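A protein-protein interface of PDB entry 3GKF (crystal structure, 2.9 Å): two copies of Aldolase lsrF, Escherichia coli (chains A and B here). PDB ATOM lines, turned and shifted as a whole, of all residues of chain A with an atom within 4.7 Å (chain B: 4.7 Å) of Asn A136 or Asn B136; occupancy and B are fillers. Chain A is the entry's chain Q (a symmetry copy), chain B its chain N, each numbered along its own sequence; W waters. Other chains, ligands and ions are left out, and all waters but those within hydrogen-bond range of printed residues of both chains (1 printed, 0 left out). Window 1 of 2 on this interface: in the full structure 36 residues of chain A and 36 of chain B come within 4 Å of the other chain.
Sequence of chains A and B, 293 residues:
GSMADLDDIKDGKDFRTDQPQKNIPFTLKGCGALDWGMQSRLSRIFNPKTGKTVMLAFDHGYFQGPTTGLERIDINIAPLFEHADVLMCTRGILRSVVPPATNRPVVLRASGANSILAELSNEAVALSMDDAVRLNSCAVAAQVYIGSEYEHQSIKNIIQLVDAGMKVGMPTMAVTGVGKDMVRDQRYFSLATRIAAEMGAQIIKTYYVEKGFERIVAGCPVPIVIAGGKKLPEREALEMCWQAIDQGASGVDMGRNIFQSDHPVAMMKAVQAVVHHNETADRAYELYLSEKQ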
ATOM      1  N   GLY A  37      33.427   9.513  26.044  1.00  0.00           N
ATOM      2  CA  GLY A  37      32.141   9.029  26.519  1.00  0.00           C
ATOM      3  C   GLY A  37      31.143  10.157  26.543  1.00  0.00           C
ATOM      4  O   GLY A  37      29.983  10.000  26.124  1.00  0.00           O
ATOM      5  N   SER A  40      30.176  11.050  23.274  1.00  0.00           N
ATOM      6  CA  SER A  40      29.344  10.003  22.732  1.00  0.00           C
ATOM      7  C   SER A  40      27.886  10.178  23.102  1.00  0.00           C
ATOM      8  O   SER A  40      27.007   9.981  22.275  1.00  0.00           O
ATOM      9  CB  SER A  40      29.826   8.631  23.212  1.00  0.00           C
ATOM     10  OG  SER A  40      29.070   7.606  22.575  1.00  0.00           O
ATOM     11  N   ARG A  41      27.647  10.498  24.371  1.00  0.00           N
ATOM     12  CA  ARG A  41      26.296  10.643  24.884  1.00  0.00           C
ATOM     13  C   ARG A  41      25.641  11.792  24.175  1.00  0.00           C
ATOM     14  O   ARG A  41      24.517  11.684  23.700  1.00  0.00           O
ATOM     15  CB  ARG A  41      26.284  10.865  26.391  1.00  0.00           C
ATOM     16  CG  ARG A  41      26.408   9.571  27.160  1.00  0.00           C
ATOM     17  CD  ARG A  41      26.681   9.781  28.644  1.00  0.00           C
ATOM     18  NE  ARG A  41      26.721   8.496  29.330  1.00  0.00           N
ATOM     19  CZ  ARG A  41      27.800   7.978  29.881  1.00  0.00           C
ATOM     20  NH1 ARG A  41      28.955   8.613  29.875  1.00  0.00           N
ATOM     21  NH2 ARG A  41      27.728   6.812  30.453  1.00  0.00           N
ATOM     22  N   ARG A  44      24.504  11.010  20.811  1.00  0.00           N
ATOM     23  CA  ARG A  44      23.232  10.263  20.785  1.00  0.00           C
ATOM     24  C   ARG A  44      22.070  11.241  20.711  1.00  0.00           C
ATOM     25  O   ARG A  44      21.102  11.025  19.985  1.00  0.00           O
ATOM     26  CB  ARG A  44      23.061   9.408  22.040  1.00  0.00           C
ATOM     27  CG  ARG A  44      23.888   8.159  22.071  1.00  0.00           C
ATOM     28  CD  ARG A  44      23.240   7.139  22.977  1.00  0.00           C
ATOM     29  NE  ARG A  44      22.236   6.379  22.237  1.00  0.00           N
ATOM     30  CZ  ARG A  44      21.345   5.552  22.783  1.00  0.00           C
ATOM     31  NH1 ARG A  44      21.295   5.367  24.100  1.00  0.00           N
ATOM     32  NH2 ARG A  44      20.489   4.912  22.000  1.00  0.00           N
ATOM     33  N   ALA A 132      21.292   7.363  37.493  1.00  0.00           N
ATOM     34  CA  ALA A 132      21.213   7.833  36.110  1.00  0.00           C
ATOM     35  C   ALA A 132      22.154   7.013  35.241  1.00  0.00           C
ATOM     36  O   ALA A 132      21.836   6.674  34.106  1.00  0.00           O
ATOM     37  CB  ALA A 132      21.570   9.275  36.014  1.00  0.00           C
ATOM     38  N   VAL A 133      23.318   6.678  35.791  1.00  0.00           N
ATOM     39  CA  VAL A 133      24.267   5.871  35.068  1.00  0.00           C
ATOM     40  C   VAL A 133      23.718   4.457  34.957  1.00  0.00           C
ATOM     41  O   VAL A 133      23.897   3.768  33.936  1.00  0.00           O
ATOM     42  CB  VAL A 133      25.586   5.833  35.800  1.00  0.00           C
ATOM     43  CG1 VAL A 133      26.428   4.611  35.359  1.00  0.00           C
ATOM     44  CG2 VAL A 133      26.295   7.102  35.574  1.00  0.00           C
ATOM     45  N   ARG A 134      23.046   4.026  36.017  1.00  0.00           N
ATOM     46  CA  ARG A 134      22.443   2.709  36.012  1.00  0.00           C
ATOM     47  C   ARG A 134      21.376   2.588  34.953  1.00  0.00           C
ATOM     48  O   ARG A 134      21.107   1.508  34.452  1.00  0.00           O
ATOM     49  CB  ARG A 134      21.835   2.375  37.365  1.00  0.00           C
ATOM     50  CG  ARG A 134      21.223   1.006  37.409  1.00  0.00           C
ATOM     51  CD  ARG A 134      20.654   0.753  38.759  1.00  0.00           C
ATOM     52  NE  ARG A 134      21.689   0.728  39.793  1.00  0.00           N
ATOM     53  CZ  ARG A 134      21.922   1.709  40.661  1.00  0.00           C
ATOM     54  NH1 ARG A 134      21.220   2.825  40.602  1.00  0.00           N
ATOM     55  NH2 ARG A 134      22.864   1.581  41.583  1.00  0.00           N
ATOM     56  N   LEU A 135      20.753   3.696  34.619  1.00  0.00           N
ATOM     57  CA  LEU A 135      19.692   3.667  33.628  1.00  0.00           C
ATOM     58  C   LEU A 135      20.195   3.987  32.234  1.00  0.00           C
ATOM     59  O   LEU A 135      19.372   4.222  31.351  1.00  0.00           O
ATOM     60  CB  LEU A 135      18.584   4.675  33.993  1.00  0.00           C
ATOM     61  CG  LEU A 135      17.659   4.232  35.143  1.00  0.00           C
ATOM     62  CD1 LEU A 135      16.728   5.329  35.549  1.00  0.00           C
ATOM     63  CD2 LEU A 135      16.867   2.968  34.771  1.00  0.00           C
ATOM     64  N   ASN A 136      21.524   4.054  32.051  1.00  0.00           N
ATOM     65  CA  ASN A 136      22.078   4.366  30.755  1.00  0.00           C
ATOM     66  C   ASN A 136      21.567   5.701  30.208  1.00  0.00           C
ATOM     67  O   ASN A 136      21.101   5.778  29.099  1.00  0.00           O
ATOM     68  CB  ASN A 136      21.627   3.274  29.804  1.00  0.00           C
ATOM     69  CG  ASN A 136      22.442   3.232  28.571  1.00  0.00           C
ATOM     70  OD1 ASN A 136      23.595   3.626  28.573  1.00  0.00           O
ATOM     71  ND2 ASN A 136      21.861   2.751  27.502  1.00  0.00           N
ATOM     72  N   SER A 137      21.599   6.763  30.973  1.00  0.00           N
ATOM     73  CA  SER A 137      21.049   8.011  30.453  1.00  0.00           C
ATOM     74  C   SER A 137      22.059   8.663  29.522  1.00  0.00           C
ATOM     75  O   SER A 137      23.249   8.378  29.607  1.00  0.00           O
ATOM     76  CB  SER A 137      20.780   9.001  31.595  1.00  0.00           C
ATOM     77  OG  SER A 137      20.075   8.402  32.670  1.00  0.00           O
ATOM     78  N   CYS A 138      21.594   9.548  28.660  1.00  0.00           N
ATOM     79  CA  CYS A 138      22.490  10.337  27.861  1.00  0.00           C
ATOM     80  C   CYS A 138      22.719  11.642  28.563  1.00  0.00           C
ATOM     81  O   CYS A 138      23.712  12.335  28.337  1.00  0.00           O
ATOM     82  CB  CYS A 138      21.863  10.638  26.517  1.00  0.00           C
ATOM     83  SG  CYS A 138      21.686   9.161  25.620  1.00  0.00           S
ATOM     84  N   GLY B  37      18.016   0.038  32.746  1.00  0.00           N
ATOM     85  CA  GLY B  37      19.258   0.495  32.149  1.00  0.00           C
ATOM     86  C   GLY B  37      19.998  -0.642  31.479  1.00  0.00           C
ATOM     87  O   GLY B  37      20.524  -0.493  30.375  1.00  0.00           O
ATOM     88  N   SER B  40      18.351  -1.679  28.498  1.00  0.00           N
ATOM     89  CA  SER B  40      18.499  -0.633  27.530  1.00  0.00           C
ATOM     90  C   SER B  40      19.804  -0.834  26.766  1.00  0.00           C
ATOM     91  O   SER B  40      19.836  -0.776  25.553  1.00  0.00           O
ATOM     92  CB  SER B  40      18.489   0.713  28.242  1.00  0.00           C
ATOM     93  OG  SER B  40      18.539   1.735  27.293  1.00  0.00           O
ATOM     94  N   ARG B  41      20.894  -1.053  27.485  1.00  0.00           N
ATOM     95  CA  ARG B  41      22.179  -1.164  26.835  1.00  0.00           C
ATOM     96  C   ARG B  41      22.154  -2.346  25.907  1.00  0.00           C
ATOM     97  O   ARG B  41      22.674  -2.255  24.795  1.00  0.00           O
ATOM     98  CB  ARG B  41      23.299  -1.343  27.841  1.00  0.00           C
ATOM     99  CG  ARG B  41      23.679  -0.077  28.506  1.00  0.00           C
ATOM    100  CD  ARG B  41      24.588  -0.319  29.704  1.00  0.00           C
ATOM    101  NE  ARG B  41      25.080   0.956  30.183  1.00  0.00           N
ATOM    102  CZ  ARG B  41      24.684   1.534  31.309  1.00  0.00           C
ATOM    103  NH1 ARG B  41      23.819   0.935  32.126  1.00  0.00           N
ATOM    104  NH2 ARG B  41      25.174   2.722  31.627  1.00  0.00           N
ATOM    105  N   ARG B  44      20.475  -1.713  22.731  1.00  0.00           N
ATOM    106  CA  ARG B  44      21.306  -0.977  21.789  1.00  0.00           C
ATOM    107  C   ARG B  44      22.069  -1.956  20.918  1.00  0.00           C
ATOM    108  O   ARG B  44      22.231  -1.759  19.726  1.00  0.00           O
ATOM    109  CB  ARG B  44      22.309  -0.107  22.535  1.00  0.00           C
ATOM    110  CG  ARG B  44      21.755   1.163  23.097  1.00  0.00           C
ATOM    111  CD  ARG B  44      22.852   2.209  23.214  1.00  0.00           C
ATOM    112  NE  ARG B  44      22.993   2.932  21.960  1.00  0.00           N
ATOM    113  CZ  ARG B  44      24.014   3.740  21.665  1.00  0.00           C
ATOM    114  NH1 ARG B  44      24.984   3.945  22.548  1.00  0.00           N
ATOM    115  NH2 ARG B  44      24.064   4.344  20.473  1.00  0.00           N
ATOM    116  N   ALA B 132      34.627   2.304  31.835  1.00  0.00           N
ATOM    117  CA  ALA B 132      33.675   1.768  30.850  1.00  0.00           C
ATOM    118  C   ALA B 132      32.409   2.605  30.906  1.00  0.00           C
ATOM    119  O   ALA B 132      31.782   2.929  29.889  1.00  0.00           O
ATOM    120  CB  ALA B 132      33.345   0.318  31.116  1.00  0.00           C
ATOM    121  N   VAL B 133      32.030   2.961  32.122  1.00  0.00           N
ATOM    122  CA  VAL B 133      30.872   3.770  32.325  1.00  0.00           C
ATOM    123  C   VAL B 133      31.162   5.163  31.813  1.00  0.00           C
ATOM    124  O   VAL B 133      30.276   5.827  31.240  1.00  0.00           O
ATOM    125  CB  VAL B 133      30.509   3.835  33.796  1.00  0.00           C
ATOM    126  CG1 VAL B 133      29.594   5.015  34.062  1.00  0.00           C
ATOM    127  CG2 VAL B 133      29.842   2.540  34.202  1.00  0.00           C
ATOM    128  N   ARG B 134      32.394   5.620  32.020  1.00  0.00           N
ATOM    129  CA  ARG B 134      32.780   6.940  31.551  1.00  0.00           C
ATOM    130  C   ARG B 134      32.731   7.016  30.064  1.00  0.00           C
ATOM    131  O   ARG B 134      32.534   8.077  29.520  1.00  0.00           O
ATOM    132  CB  ARG B 134      34.201   7.260  31.970  1.00  0.00           C
ATOM    133  CG  ARG B 134      34.672   8.640  31.561  1.00  0.00           C
ATOM    134  CD  ARG B 134      36.027   8.970  32.140  1.00  0.00           C
ATOM    135  NE  ARG B 134      36.015   9.029  33.599  1.00  0.00           N
ATOM    136  CZ  ARG B 134      36.442   8.051  34.400  1.00  0.00           C
ATOM    137  NH1 ARG B 134      36.925   6.914  33.886  1.00  0.00           N
ATOM    138  NH2 ARG B 134      36.396   8.209  35.722  1.00  0.00           N
ATOM    139  N   LEU B 135      32.946   5.893  29.404  1.00  0.00           N
ATOM    140  CA  LEU B 135      32.982   5.871  27.949  1.00  0.00           C
ATOM    141  C   LEU B 135      31.632   5.519  27.331  1.00  0.00           C
ATOM    142  O   LEU B 135      31.540   5.235  26.136  1.00  0.00           O
ATOM    143  CB  LEU B 135      34.027   4.876  27.460  1.00  0.00           C
ATOM    144  CG  LEU B 135      35.479   5.334  27.588  1.00  0.00           C
ATOM    145  CD1 LEU B 135      36.443   4.241  27.202  1.00  0.00           C
ATOM    146  CD2 LEU B 135      35.743   6.567  26.769  1.00  0.00           C
ATOM    147  N   ASN B 136      30.597   5.502  28.151  1.00  0.00           N
ATOM    148  CA  ASN B 136      29.292   5.146  27.661  1.00  0.00           C
ATOM    149  C   ASN B 136      29.205   3.802  26.968  1.00  0.00           C
ATOM    150  O   ASN B 136      28.608   3.726  25.913  1.00  0.00           O
ATOM    151  CB  ASN B 136      28.880   6.187  26.651  1.00  0.00           C
ATOM    152  CG  ASN B 136      27.403   6.249  26.476  1.00  0.00           C
ATOM    153  OD1 ASN B 136      26.642   5.916  27.388  1.00  0.00           O
ATOM    154  ND2 ASN B 136      26.975   6.691  25.312  1.00  0.00           N
ATOM    155  N   SER B 137      29.785   2.743  27.531  1.00  0.00           N
ATOM    156  CA  SER B 137      29.774   1.448  26.854  1.00  0.00           C
ATOM    157  C   SER B 137      28.433   0.794  26.983  1.00  0.00           C
ATOM    158  O   SER B 137      27.675   1.065  27.914  1.00  0.00           O
ATOM    159  CB  SER B 137      30.787   0.516  27.462  1.00  0.00           C
ATOM    160  OG  SER B 137      32.026   1.181  27.597  1.00  0.00           O
ATOM    161  N   CYS B 138      28.133  -0.076  26.038  1.00  0.00           N
ATOM    162  CA  CYS B 138      26.951  -0.894  26.126  1.00  0.00           C
ATOM    163  C   CYS B 138      27.276  -2.199  26.816  1.00  0.00           C
ATOM    164  O   CYS B 138      26.393  -2.878  27.354  1.00  0.00           O
ATOM    165  CB  CYS B 138      26.444  -1.177  24.735  1.00  0.00           C
ATOM    166  SG  CYS B 138      25.782   0.306  23.996  1.00  0.00           S
HETATM  167  O   HOH W   1      20.203  -0.804  34.492  1.00  0.00           O
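Of the printed residues of chain B, Asn A136 touches Gly B37, Ser B40, Arg B41 and Asn B136. Of the printed residues of chain A, Asn B136 touches Ser A40 (3.6 Å), Arg A41 (3.2 Å) and Asn A136 (3.99 Å). Printed residues of chain A within 4 Å of Arg B134: Gly A37 (3.2 Å) and Arg A41 (3.6 Å). Printed residues of chain A within 4 Å of Ser B40: Asn A136. Of the printed residues of chain B, Leu A135 touches Gly B37. Cys B138 touches none of the printed residues of chain A.
NE of Arg A41 is in hydrogen-bond range of O of Ser A137, at 3.5 Å. NE of Arg B41 lies within hydrogen-bond range of O of Ser B137, 3.4 Å away.
Printed residues of chain B that touch a printed residue of chain A: Gly B37, Ser B40, Arg B41, Arg B44, Val B133, Arg B134, Leu B135 and Asn B136. Of the 11 printed residues of chain A, 8 touch a printed residue of chain B. Printed residues of chain A that touch a printed residue of chain B: Gly A37, Ser A40, Arg A41, Arg A44, Val A133, Arg A134, Leu A135 and Asn A136. Along chain A the printed residues that touch a printed residue of chain B span positions 37 to 136. Among the printed residues, no Asp or Glu carboxylate lies within 4 Å of a Lys or Arg side-chain nitrogen of the other chain.
Among the printed residues, merely in contact across the chains: Gly A37 with Arg B134, Gly A37 with Leu B135, Ser A40 with Asn B136, Arg A41 with Arg B134, Val A133 with Val B133, Arg A134 with Gly B37, Arg A134 with Arg B41, Leu A135 with Gly B37, Asn A136 with Gly B37 and Asn A136 with Asn B136.
OG of Ser B40 is in hydrogen-bond range of ND2 of Asn A136. The guanidinium group (NH2) of Arg A44 lies close to the guanidinium group (NE) of Arg B44 (3.2 Å). The guanidinium group (NE) of Arg B41 sits at hydrogen-bond distance from the side-chain amide oxygen (OD1) of Asn A136, at 3.5 Å. O of Val B133 lies within hydrogen-bond range of NH2 of Arg A41, at 2.8 Å. OD1 of Asn B136 sits at hydrogen-bond distance from NE of Arg A41 (3.2 Å). The guanidinium group (NH2) of Arg B41 sits at hydrogen-bond distance from the backbone carbonyl oxygen (O) of Val A133 (2.8 Å).
Water W1 bridges the backbone carbonyl oxygen (O) of Arg A134 (2.5 Å) and the backbone NH (N) of Gly B37 (2.9 Å).
Gly A37 touches Leu B135, and with the chains exchanged Leu A135 touches Gly B37. Arg A41 touches Val B133, and with the chains exchanged Val A133 touches Arg B41. Arg A41 touches Arg B134, and with the chains exchanged Arg A134 touches Arg B41. Val B133 touches its own counterpart, Val A133. Positions printed for both chains: 37, 40, 41, 44, 132, 133, 134, 135, 136, 137 and 138.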
